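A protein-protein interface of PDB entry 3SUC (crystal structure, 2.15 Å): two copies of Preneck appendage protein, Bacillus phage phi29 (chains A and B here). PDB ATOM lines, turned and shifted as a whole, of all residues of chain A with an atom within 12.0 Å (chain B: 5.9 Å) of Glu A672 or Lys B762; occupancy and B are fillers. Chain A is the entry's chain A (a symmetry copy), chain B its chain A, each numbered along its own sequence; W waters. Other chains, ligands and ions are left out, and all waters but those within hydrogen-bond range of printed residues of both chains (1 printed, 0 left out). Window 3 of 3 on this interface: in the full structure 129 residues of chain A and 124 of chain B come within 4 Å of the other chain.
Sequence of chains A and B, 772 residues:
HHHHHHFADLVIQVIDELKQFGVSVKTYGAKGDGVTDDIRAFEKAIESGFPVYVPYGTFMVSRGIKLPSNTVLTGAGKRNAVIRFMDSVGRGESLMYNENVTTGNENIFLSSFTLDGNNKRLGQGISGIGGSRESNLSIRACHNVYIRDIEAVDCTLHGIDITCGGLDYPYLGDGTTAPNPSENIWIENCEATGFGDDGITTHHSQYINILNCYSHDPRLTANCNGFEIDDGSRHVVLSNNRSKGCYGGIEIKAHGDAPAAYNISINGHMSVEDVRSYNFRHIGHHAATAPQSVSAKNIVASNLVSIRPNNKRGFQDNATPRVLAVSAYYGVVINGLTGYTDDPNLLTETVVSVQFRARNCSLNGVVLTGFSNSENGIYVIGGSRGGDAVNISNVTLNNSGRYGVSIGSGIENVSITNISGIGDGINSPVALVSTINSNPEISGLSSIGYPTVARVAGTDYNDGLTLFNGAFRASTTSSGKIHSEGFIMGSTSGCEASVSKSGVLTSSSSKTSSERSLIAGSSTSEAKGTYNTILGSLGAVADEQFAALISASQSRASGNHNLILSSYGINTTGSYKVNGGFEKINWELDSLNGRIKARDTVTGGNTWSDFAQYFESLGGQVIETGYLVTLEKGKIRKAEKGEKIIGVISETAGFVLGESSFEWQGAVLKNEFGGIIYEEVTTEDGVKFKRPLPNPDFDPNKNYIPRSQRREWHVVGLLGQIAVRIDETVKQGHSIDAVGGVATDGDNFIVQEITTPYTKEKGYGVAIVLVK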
ATOM      1  N   GLN A 665     -33.803   6.092  14.831  1.00  0.00           N
ATOM      2  CA  GLN A 665     -33.311   5.930  13.463  1.00  0.00           C
ATOM      3  C   GLN A 665     -31.943   6.583  13.198  1.00  0.00           C
ATOM      4  O   GLN A 665     -31.142   6.065  12.407  1.00  0.00           O
ATOM      5  CB  GLN A 665     -34.367   6.392  12.450  1.00  0.00           C
ATOM      6  CG  GLN A 665     -34.735   7.876  12.500  1.00  0.00           C
ATOM      7  CD  GLN A 665     -33.902   8.728  11.551  1.00  0.00           C
ATOM      8  OE1 GLN A 665     -33.588   9.882  11.850  1.00  0.00           O
ATOM      9  NE2 GLN A 665     -33.545   8.165  10.399  1.00  0.00           N
ATOM     10  N   VAL A 668     -27.171   5.818  14.399  1.00  0.00           N
ATOM     11  CA  VAL A 668     -26.034   5.266  13.670  1.00  0.00           C
ATOM     12  C   VAL A 668     -25.695   6.144  12.461  1.00  0.00           C
ATOM     13  O   VAL A 668     -26.593   6.704  11.825  1.00  0.00           O
ATOM     14  CB  VAL A 668     -26.327   3.796  13.246  1.00  0.00           C
ATOM     15  CG1 VAL A 668     -25.542   3.387  12.008  1.00  0.00           C
ATOM     16  CG2 VAL A 668     -26.051   2.846  14.398  1.00  0.00           C
ATOM     17  N   LEU A 669     -24.403   6.267  12.154  1.00  0.00           N
ATOM     18  CA  LEU A 669     -23.950   7.037  10.994  1.00  0.00           C
ATOM     19  C   LEU A 669     -24.211   6.338   9.664  1.00  0.00           C
ATOM     20  O   LEU A 669     -23.854   5.171   9.469  1.00  0.00           O
ATOM     21  CB  LEU A 669     -22.470   7.409  11.111  1.00  0.00           C
ATOM     22  CG  LEU A 669     -22.078   8.510  12.107  1.00  0.00           C
ATOM     23  CD1 LEU A 669     -20.577   8.776  12.024  1.00  0.00           C
ATOM     24  CD2 LEU A 669     -22.873   9.796  11.879  1.00  0.00           C
ATOM     25  N   LYS A 670     -24.827   7.081   8.754  1.00  0.00           N
ATOM     26  CA  LYS A 670     -25.187   6.582   7.436  1.00  0.00           C
ATOM     27  C   LYS A 670     -24.574   7.463   6.357  1.00  0.00           C
ATOM     28  O   LYS A 670     -24.443   8.680   6.534  1.00  0.00           O
ATOM     29  CB  LYS A 670     -26.712   6.565   7.267  1.00  0.00           C
ATOM     30  CG  LYS A 670     -27.458   5.585   8.167  1.00  0.00           C
ATOM     31  CD  LYS A 670     -28.904   6.043   8.354  1.00  0.00           C
ATOM     32  CE  LYS A 670     -29.860   4.889   8.619  1.00  0.00           C
ATOM     33  NZ  LYS A 670     -29.615   4.204   9.917  1.00  0.00           N
ATOM     34  N   ASN A 671     -24.209   6.847   5.236  1.00  0.00           N
ATOM     35  CA  ASN A 671     -23.708   7.582   4.087  1.00  0.00           C
ATOM     36  C   ASN A 671     -24.837   8.309   3.351  1.00  0.00           C
ATOM     37  O   ASN A 671     -25.996   8.280   3.784  1.00  0.00           O
ATOM     38  CB  ASN A 671     -22.897   6.664   3.154  1.00  0.00           C
ATOM     39  CG  ASN A 671     -23.722   5.523   2.562  1.00  0.00           C
ATOM     40  OD1 ASN A 671     -24.787   5.736   1.986  1.00  0.00           O
ATOM     41  ND2 ASN A 671     -23.205   4.310   2.669  1.00  0.00           N
ATOM     42  N   GLU A 672     -24.495   8.953   2.238  1.00  0.00           N
ATOM     43  CA  GLU A 672     -25.456   9.734   1.451  1.00  0.00           C
ATOM     44  C   GLU A 672     -26.597   8.901   0.846  1.00  0.00           C
ATOM     45  O   GLU A 672     -27.639   9.449   0.477  1.00  0.00           O
ATOM     46  CB  GLU A 672     -24.737  10.525   0.353  1.00  0.00           C
ATOM     47  CG  GLU A 672     -23.982   9.663  -0.653  1.00  0.00           C
ATOM     48  CD  GLU A 672     -23.373  10.467  -1.786  1.00  0.00           C
ATOM     49  OE1 GLU A 672     -22.582   9.888  -2.567  1.00  0.00           O
ATOM     50  OE2 GLU A 672     -23.685  11.675  -1.898  1.00  0.00           O
ATOM     51  N   PHE A 673     -26.386   7.590   0.739  1.00  0.00           N
ATOM     52  CA  PHE A 673     -27.393   6.678   0.195  1.00  0.00           C
ATOM     53  C   PHE A 673     -28.194   5.956   1.285  1.00  0.00           C
ATOM     54  O   PHE A 673     -29.066   5.138   0.985  1.00  0.00           O
ATOM     55  CB  PHE A 673     -26.749   5.686  -0.776  1.00  0.00           C
ATOM     56  CG  PHE A 673     -26.162   6.336  -1.993  1.00  0.00           C
ATOM     57  CD1 PHE A 673     -26.983   6.814  -3.005  1.00  0.00           C
ATOM     58  CD2 PHE A 673     -24.786   6.479  -2.124  1.00  0.00           C
ATOM     59  CE1 PHE A 673     -26.444   7.423  -4.130  1.00  0.00           C
ATOM     60  CE2 PHE A 673     -24.238   7.087  -3.250  1.00  0.00           C
ATOM     61  CZ  PHE A 673     -25.070   7.560  -4.251  1.00  0.00           C
ATOM     62  N   GLY A 674     -27.900   6.280   2.544  1.00  0.00           N
ATOM     63  CA  GLY A 674     -28.603   5.718   3.695  1.00  0.00           C
ATOM     64  C   GLY A 674     -27.931   4.484   4.255  1.00  0.00           C
ATOM     65  O   GLY A 674     -28.408   3.900   5.234  1.00  0.00           O
ATOM     66  N   GLY A 675     -26.824   4.087   3.632  1.00  0.00           N
ATOM     67  CA  GLY A 675     -26.084   2.894   4.032  1.00  0.00           C
ATOM     68  C   GLY A 675     -25.248   3.157   5.266  1.00  0.00           C
ATOM     69  O   GLY A 675     -24.678   4.235   5.413  1.00  0.00           O
ATOM     70  N   ILE A 676     -25.175   2.165   6.149  1.00  0.00           N
ATOM     71  CA  ILE A 676     -24.434   2.287   7.400  1.00  0.00           C
ATOM     72  C   ILE A 676     -22.921   2.358   7.150  1.00  0.00           C
ATOM     73  O   ILE A 676     -22.376   1.611   6.331  1.00  0.00           O
ATOM     74  CB  ILE A 676     -24.795   1.135   8.377  1.00  0.00           C
ATOM     75  CG1 ILE A 676     -26.269   1.237   8.790  1.00  0.00           C
ATOM     76  CG2 ILE A 676     -23.897   1.144   9.613  1.00  0.00           C
ATOM     77  CD1 ILE A 676     -26.795   0.041   9.571  1.00  0.00           C
ATOM     78  N   ILE A 677     -22.256   3.280   7.841  1.00  0.00           N
ATOM     79  CA  ILE A 677     -20.796   3.336   7.816  1.00  0.00           C
ATOM     80  C   ILE A 677     -20.249   2.518   8.985  1.00  0.00           C
ATOM     81  O   ILE A 677     -20.787   2.558  10.096  1.00  0.00           O
ATOM     82  CB  ILE A 677     -20.243   4.786   7.828  1.00  0.00           C
ATOM     83  CG1 ILE A 677     -21.013   5.668   6.838  1.00  0.00           C
ATOM     84  CG2 ILE A 677     -18.754   4.784   7.474  1.00  0.00           C
ATOM     85  CD1 ILE A 677     -20.947   7.155   7.127  1.00  0.00           C
ATOM     86  N   TYR A 678     -19.178   1.774   8.716  1.00  0.00           N
ATOM     87  CA  TYR A 678     -18.632   0.821   9.672  1.00  0.00           C
ATOM     88  C   TYR A 678     -17.178   1.102  10.037  1.00  0.00           C
ATOM     89  O   TYR A 678     -16.469   1.823   9.325  1.00  0.00           O
ATOM     90  CB  TYR A 678     -18.742  -0.605   9.114  1.00  0.00           C
ATOM     91  CG  TYR A 678     -20.161  -1.105   8.950  1.00  0.00           C
ATOM     92  CD1 TYR A 678     -20.817  -1.016   7.721  1.00  0.00           C
ATOM     93  CD2 TYR A 678     -20.845  -1.668  10.020  1.00  0.00           C
ATOM     94  CE1 TYR A 678     -22.118  -1.474   7.569  1.00  0.00           C
ATOM     95  CE2 TYR A 678     -22.146  -2.132   9.884  1.00  0.00           C
ATOM     96  CZ  TYR A 678     -22.779  -2.035   8.656  1.00  0.00           C
ATOM     97  OH  TYR A 678     -24.072  -2.499   8.525  1.00  0.00           O
ATOM     98  N   LEU A 693     -20.972   2.797  13.040  1.00  0.00           N
ATOM     99  CA  LEU A 693     -20.487   4.031  13.656  1.00  0.00           C
ATOM    100  C   LEU A 693     -21.582   4.784  14.409  1.00  0.00           C
ATOM    101  O   LEU A 693     -22.645   5.053  13.853  1.00  0.00           O
ATOM    102  CB  LEU A 693     -19.852   4.943  12.601  1.00  0.00           C
ATOM    103  CG  LEU A 693     -18.326   5.050  12.485  1.00  0.00           C
ATOM    104  CD1 LEU A 693     -17.631   3.706  12.515  1.00  0.00           C
ATOM    105  CD2 LEU A 693     -17.959   5.800  11.219  1.00  0.00           C
ATOM    106  N   TRP B 608     -34.689   4.040   5.732  1.00  0.00           N
ATOM    107  CA  TRP B 608     -35.246   3.744   4.410  1.00  0.00           C
ATOM    108  C   TRP B 608     -34.653   2.463   3.827  1.00  0.00           C
ATOM    109  O   TRP B 608     -33.430   2.311   3.695  1.00  0.00           O
ATOM    110  CB  TRP B 608     -35.232   4.939   3.426  1.00  0.00           C
ATOM    111  CG  TRP B 608     -33.924   5.639   3.226  1.00  0.00           C
ATOM    112  CD1 TRP B 608     -32.843   5.184   2.519  1.00  0.00           C
ATOM    113  CD2 TRP B 608     -33.572   6.947   3.703  1.00  0.00           C
ATOM    114  NE1 TRP B 608     -31.833   6.119   2.545  1.00  0.00           N
ATOM    115  CE2 TRP B 608     -32.249   7.209   3.265  1.00  0.00           C
ATOM    116  CE3 TRP B 608     -34.240   7.917   4.465  1.00  0.00           C
ATOM    117  CZ2 TRP B 608     -31.581   8.408   3.561  1.00  0.00           C
ATOM    118  CZ3 TRP B 608     -33.575   9.108   4.766  1.00  0.00           C
ATOM    119  CH2 TRP B 608     -32.255   9.343   4.311  1.00  0.00           C
ATOM    120  N   ALA B 723     -32.659   5.231  -2.261  1.00  0.00           N
ATOM    121  CA  ALA B 723     -31.763   6.345  -2.585  1.00  0.00           C
ATOM    122  C   ALA B 723     -31.232   6.217  -4.009  1.00  0.00           C
ATOM    123  O   ALA B 723     -30.696   5.172  -4.397  1.00  0.00           O
ATOM    124  CB  ALA B 723     -30.620   6.418  -1.588  1.00  0.00           C
ATOM    125  N   ARG B 725     -29.127   8.344  -7.351  1.00  0.00           N
ATOM    126  CA  ARG B 725     -28.328   9.420  -7.944  1.00  0.00           C
ATOM    127  C   ARG B 725     -29.148  10.189  -8.972  1.00  0.00           C
ATOM    128  O   ARG B 725     -29.683   9.599  -9.912  1.00  0.00           O
ATOM    129  CB  ARG B 725     -27.080   8.855  -8.630  1.00  0.00           C
ATOM    130  CG  ARG B 725     -26.113   8.177  -7.696  1.00  0.00           C
ATOM    131  CD  ARG B 725     -25.186   7.235  -8.433  1.00  0.00           C
ATOM    132  NE  ARG B 725     -24.274   6.576  -7.495  1.00  0.00           N
ATOM    133  CZ  ARG B 725     -23.081   7.056  -7.130  1.00  0.00           C
ATOM    134  NH1 ARG B 725     -22.636   8.204  -7.629  1.00  0.00           N
ATOM    135  NH2 ARG B 725     -22.332   6.387  -6.261  1.00  0.00           N
ATOM    136  N   THR B 755     -32.516  14.535  -0.826  1.00  0.00           N
ATOM    137  CA  THR B 755     -31.852  14.509   0.477  1.00  0.00           C
ATOM    138  C   THR B 755     -30.428  15.055   0.382  1.00  0.00           C
ATOM    139  O   THR B 755     -29.827  15.425   1.393  1.00  0.00           O
ATOM    140  CB  THR B 755     -31.831  13.083   1.078  1.00  0.00           C
ATOM    141  OG1 THR B 755     -31.201  12.178   0.160  1.00  0.00           O
ATOM    142  CG2 THR B 755     -33.247  12.605   1.374  1.00  0.00           C
ATOM    143  N   THR B 756     -29.902  15.076  -0.841  1.00  0.00           N
ATOM    144  CA  THR B 756     -28.626  15.698  -1.167  1.00  0.00           C
ATOM    145  C   THR B 756     -28.790  16.368  -2.528  1.00  0.00           C
ATOM    146  O   THR B 756     -28.779  15.690  -3.558  1.00  0.00           O
ATOM    147  CB  THR B 756     -27.472  14.669  -1.193  1.00  0.00           C
ATOM    148  OG1 THR B 756     -27.326  14.094   0.107  1.00  0.00           O
ATOM    149  CG2 THR B 756     -26.150  15.317  -1.589  1.00  0.00           C
ATOM    150  N   PRO B 757     -28.970  17.705  -2.534  1.00  0.00           N
ATOM    151  CA  PRO B 757     -29.223  18.444  -3.771  1.00  0.00           C
ATOM    152  C   PRO B 757     -28.079  18.323  -4.771  1.00  0.00           C
ATOM    153  O   PRO B 757     -26.917  18.221  -4.370  1.00  0.00           O
ATOM    154  CB  PRO B 757     -29.364  19.894  -3.292  1.00  0.00           C
ATOM    155  CG  PRO B 757     -29.700  19.792  -1.852  1.00  0.00           C
ATOM    156  CD  PRO B 757     -28.953  18.599  -1.362  1.00  0.00           C
ATOM    157  N   THR B 759     -25.117  19.034  -7.271  1.00  0.00           N
ATOM    158  CA  THR B 759     -24.047  20.016  -7.424  1.00  0.00           C
ATOM    159  C   THR B 759     -23.231  19.669  -8.661  1.00  0.00           C
ATOM    160  O   THR B 759     -22.942  18.492  -8.912  1.00  0.00           O
ATOM    161  CB  THR B 759     -23.101  20.054  -6.211  1.00  0.00           C
ATOM    162  OG1 THR B 759     -22.529  18.757  -6.014  1.00  0.00           O
ATOM    163  CG2 THR B 759     -23.832  20.493  -4.943  1.00  0.00           C
ATOM    164  N   LYS B 760     -22.874  20.701  -9.427  1.00  0.00           N
ATOM    165  CA  LYS B 760     -21.993  20.585 -10.597  1.00  0.00           C
ATOM    166  C   LYS B 760     -20.722  19.790 -10.296  1.00  0.00           C
ATOM    167  O   LYS B 760     -20.272  18.986 -11.115  1.00  0.00           O
ATOM    168  CB  LYS B 760     -21.591  21.976 -11.105  1.00  0.00           C
ATOM    169  CG  LYS B 760     -22.661  22.712 -11.885  1.00  0.00           C
ATOM    170  CD  LYS B 760     -22.283  24.188 -12.068  1.00  0.00           C
ATOM    171  CE  LYS B 760     -23.421  25.006 -12.714  1.00  0.00           C
ATOM    172  NZ  LYS B 760     -23.440  24.952 -14.213  1.00  0.00           N
ATOM    173  N   GLU B 761     -20.156  20.027  -9.120  1.00  0.00           N
ATOM    174  CA  GLU B 761     -18.871  19.454  -8.734  1.00  0.00           C
ATOM    175  C   GLU B 761     -18.923  17.947  -8.481  1.00  0.00           C
ATOM    176  O   GLU B 761     -18.004  17.214  -8.869  1.00  0.00           O
ATOM    177  CB  GLU B 761     -18.273  20.204  -7.534  1.00  0.00           C
ATOM    178  CG  GLU B 761     -19.300  20.884  -6.631  1.00  0.00           C
ATOM    179  CD  GLU B 761     -19.690  22.290  -7.094  1.00  0.00           C
ATOM    180  OE1 GLU B 761     -18.800  23.149  -7.245  1.00  0.00           O
ATOM    181  OE2 GLU B 761     -20.899  22.542  -7.284  1.00  0.00           O
ATOM    182  N   LYS B 762     -19.996  17.488  -7.836  1.00  0.00           N
ATOM    183  CA  LYS B 762     -20.182  16.056  -7.617  1.00  0.00           C
ATOM    184  C   LYS B 762     -20.668  15.354  -8.885  1.00  0.00           C
ATOM    185  O   LYS B 762     -20.239  14.238  -9.190  1.00  0.00           O
ATOM    186  CB  LYS B 762     -21.126  15.785  -6.450  1.00  0.00           C
ATOM    187  CG  LYS B 762     -20.486  15.972  -5.081  1.00  0.00           C
ATOM    188  CD  LYS B 762     -20.994  14.936  -4.082  1.00  0.00           C
ATOM    189  CE  LYS B 762     -22.488  15.079  -3.823  1.00  0.00           C
ATOM    190  NZ  LYS B 762     -23.043  13.863  -3.175  1.00  0.00           N
ATOM    191  N   GLY B 763     -21.543  16.028  -9.627  1.00  0.00           N
ATOM    192  CA  GLY B 763     -22.076  15.489 -10.872  1.00  0.00           C
ATOM    193  C   GLY B 763     -23.391  14.768 -10.659  1.00  0.00           C
ATOM    194  O   GLY B 763     -23.976  14.238 -11.603  1.00  0.00           O
ATOM    195  N   TYR B 764     -23.849  14.750  -9.409  1.00  0.00           N
ATOM    196  CA  TYR B 764     -25.117  14.129  -9.042  1.00  0.00           C
ATOM    197  C   TYR B 764     -25.604  14.633  -7.690  1.00  0.00           C
ATOM    198  O   TYR B 764     -24.827  15.180  -6.901  1.00  0.00           O
ATOM    199  CB  TYR B 764     -24.986  12.598  -9.004  1.00  0.00           C
ATOM    200  CG  TYR B 764     -24.132  12.081  -7.869  1.00  0.00           C
ATOM    201  CD1 TYR B 764     -22.738  11.994  -7.996  1.00  0.00           C
ATOM    202  CD2 TYR B 764     -24.712  11.682  -6.664  1.00  0.00           C
ATOM    203  CE1 TYR B 764     -21.947  11.523  -6.952  1.00  0.00           C
ATOM    204  CE2 TYR B 764     -23.933  11.215  -5.614  1.00  0.00           C
ATOM    205  CZ  TYR B 764     -22.551  11.136  -5.763  1.00  0.00           C
ATOM    206  OH  TYR B 764     -21.785  10.663  -4.719  1.00  0.00           O
ATOM    207  N   GLY B 765     -26.898  14.442  -7.444  1.00  0.00           N
ATOM    208  CA  GLY B 765     -27.469  14.551  -6.110  1.00  0.00           C
ATOM    209  C   GLY B 765     -28.046  13.213  -5.669  1.00  0.00           C
ATOM    210  O   GLY B 765     -27.929  12.205  -6.375  1.00  0.00           O
ATOM    211  N   VAL B 766     -28.660  13.194  -4.491  1.00  0.00           N
ATOM    212  CA  VAL B 766     -29.347  12.003  -4.011  1.00  0.00           C
ATOM    213  C   VAL B 766     -30.797  12.313  -3.622  1.00  0.00           C
ATOM    214  O   VAL B 766     -31.072  13.234  -2.851  1.00  0.00           O
ATOM    215  CB  VAL B 766     -28.596  11.320  -2.832  1.00  0.00           C
ATOM    216  CG1 VAL B 766     -29.276  10.006  -2.455  1.00  0.00           C
ATOM    217  CG2 VAL B 766     -27.127  11.060  -3.192  1.00  0.00           C
HETATM  218  O   HOH W   1     -31.323   3.878   5.845  1.00  0.00           O
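OE1 of Glu A672 sits at hydrogen-bond distance from OH of Tyr B764 (2.4 Å).
The backbone carbonyl oxygen (O) of Phe A673 is in hydrogen-bond range of the indole nitrogen (NE1) of Trp B608, at 3.3 Å.
OE2 of Glu A672 lies within salt-bridge range of NZ of Lys B762 (2.6 Å).
OD1 of Asn A671 is in hydrogen-bond range of N of Phe A673 (2.7 Å).
The backbone NH (N) of Gly A674 is in hydrogen-bond range of the side-chain amide oxygen (OD1) of Asn A671 (3.2 Å).
The backbone carbonyl oxygen (O) of Val B766 is in hydrogen-bond range of the backbone NH (N) of Thr B755, at 2.8 Å.
The side-chain hydroxyl of Thr B759 lies close to the backbone NH of Lys B762 (3.4 Å).
The backbone carbonyl oxygen of Thr B756 lies within hydrogen-bond range of the backbone NH of Val B766, 2.7 Å away.
Among the printed residues, merely in contact across the chains: Phe A673 with Ala B723, Glu A672 with Val B766, Gly A674 with Trp B608, Phe A673 with Arg B725 and Phe A673 with Val B766.
Glu A672 touches just these residues of chain B: Lys B762, Tyr B764 and Val B766.
Of the printed residues of chain B, Phe A673 touches Trp B608 (3.3 Å), Ala B723 (3.3 Å), Arg B725 (3.5 Å) and Val B766 (3.8 Å).
Gly A675 touches none of the printed residues of chain B.
Ile A676 touches none of the printed residues of chain B.
Printed residues of chain A within 4 Å of Arg B725: Phe A673.
No residue of chain A comes within 4 Å of Thr B755.
No residue of chain A comes within 4 Å of Thr B756.
No residue of chain A comes within 4 Å of Thr B759.
Lys B762 touches just one residue of chain A: Glu A672 (2.6 Å).
No residue of chain A comes within 4 Å of Gly B763.
Of chain A, only Glu A672 comes within 4 Å of Tyr B764.
Val B766 touches two residues of chain A.
The nearest residue of chain A that does not touch Lys B762 is Phe A673 (6.7 Å).
The nearest printed residue of chain A that does not touch Trp B608 is Glu A672 (5.1 Å).
Printed residues of chain B that touch a printed residue of chain A: Trp B608, Ala B723, Arg B725, Lys B762, Tyr B764 and Val B766.
Along chain B the printed residues that touch a printed residue of chain A span positions 608 to 766.
Hydrophobic or aromatic side chains of chain A that line the printed part of chain B: Phe A673.
Among the printed residues, 8 pairs touch across the chains.
Among the printed residues, Asp or Glu carboxylates within 4 Å of a Lys or Arg side-chain nitrogen of the other chain: Glu A672 with Lys B762.
No position is printed for both chains.
Of the 8 pairs that touch across the chains among the printed residues, none has its exchanged pair printed and touching as well.
Water W1 bridges the backbone carbonyl oxygen (O) of Gly A674 (3.0 Å) and the backbone NH (N) of Trp B608 (3.4 Å).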
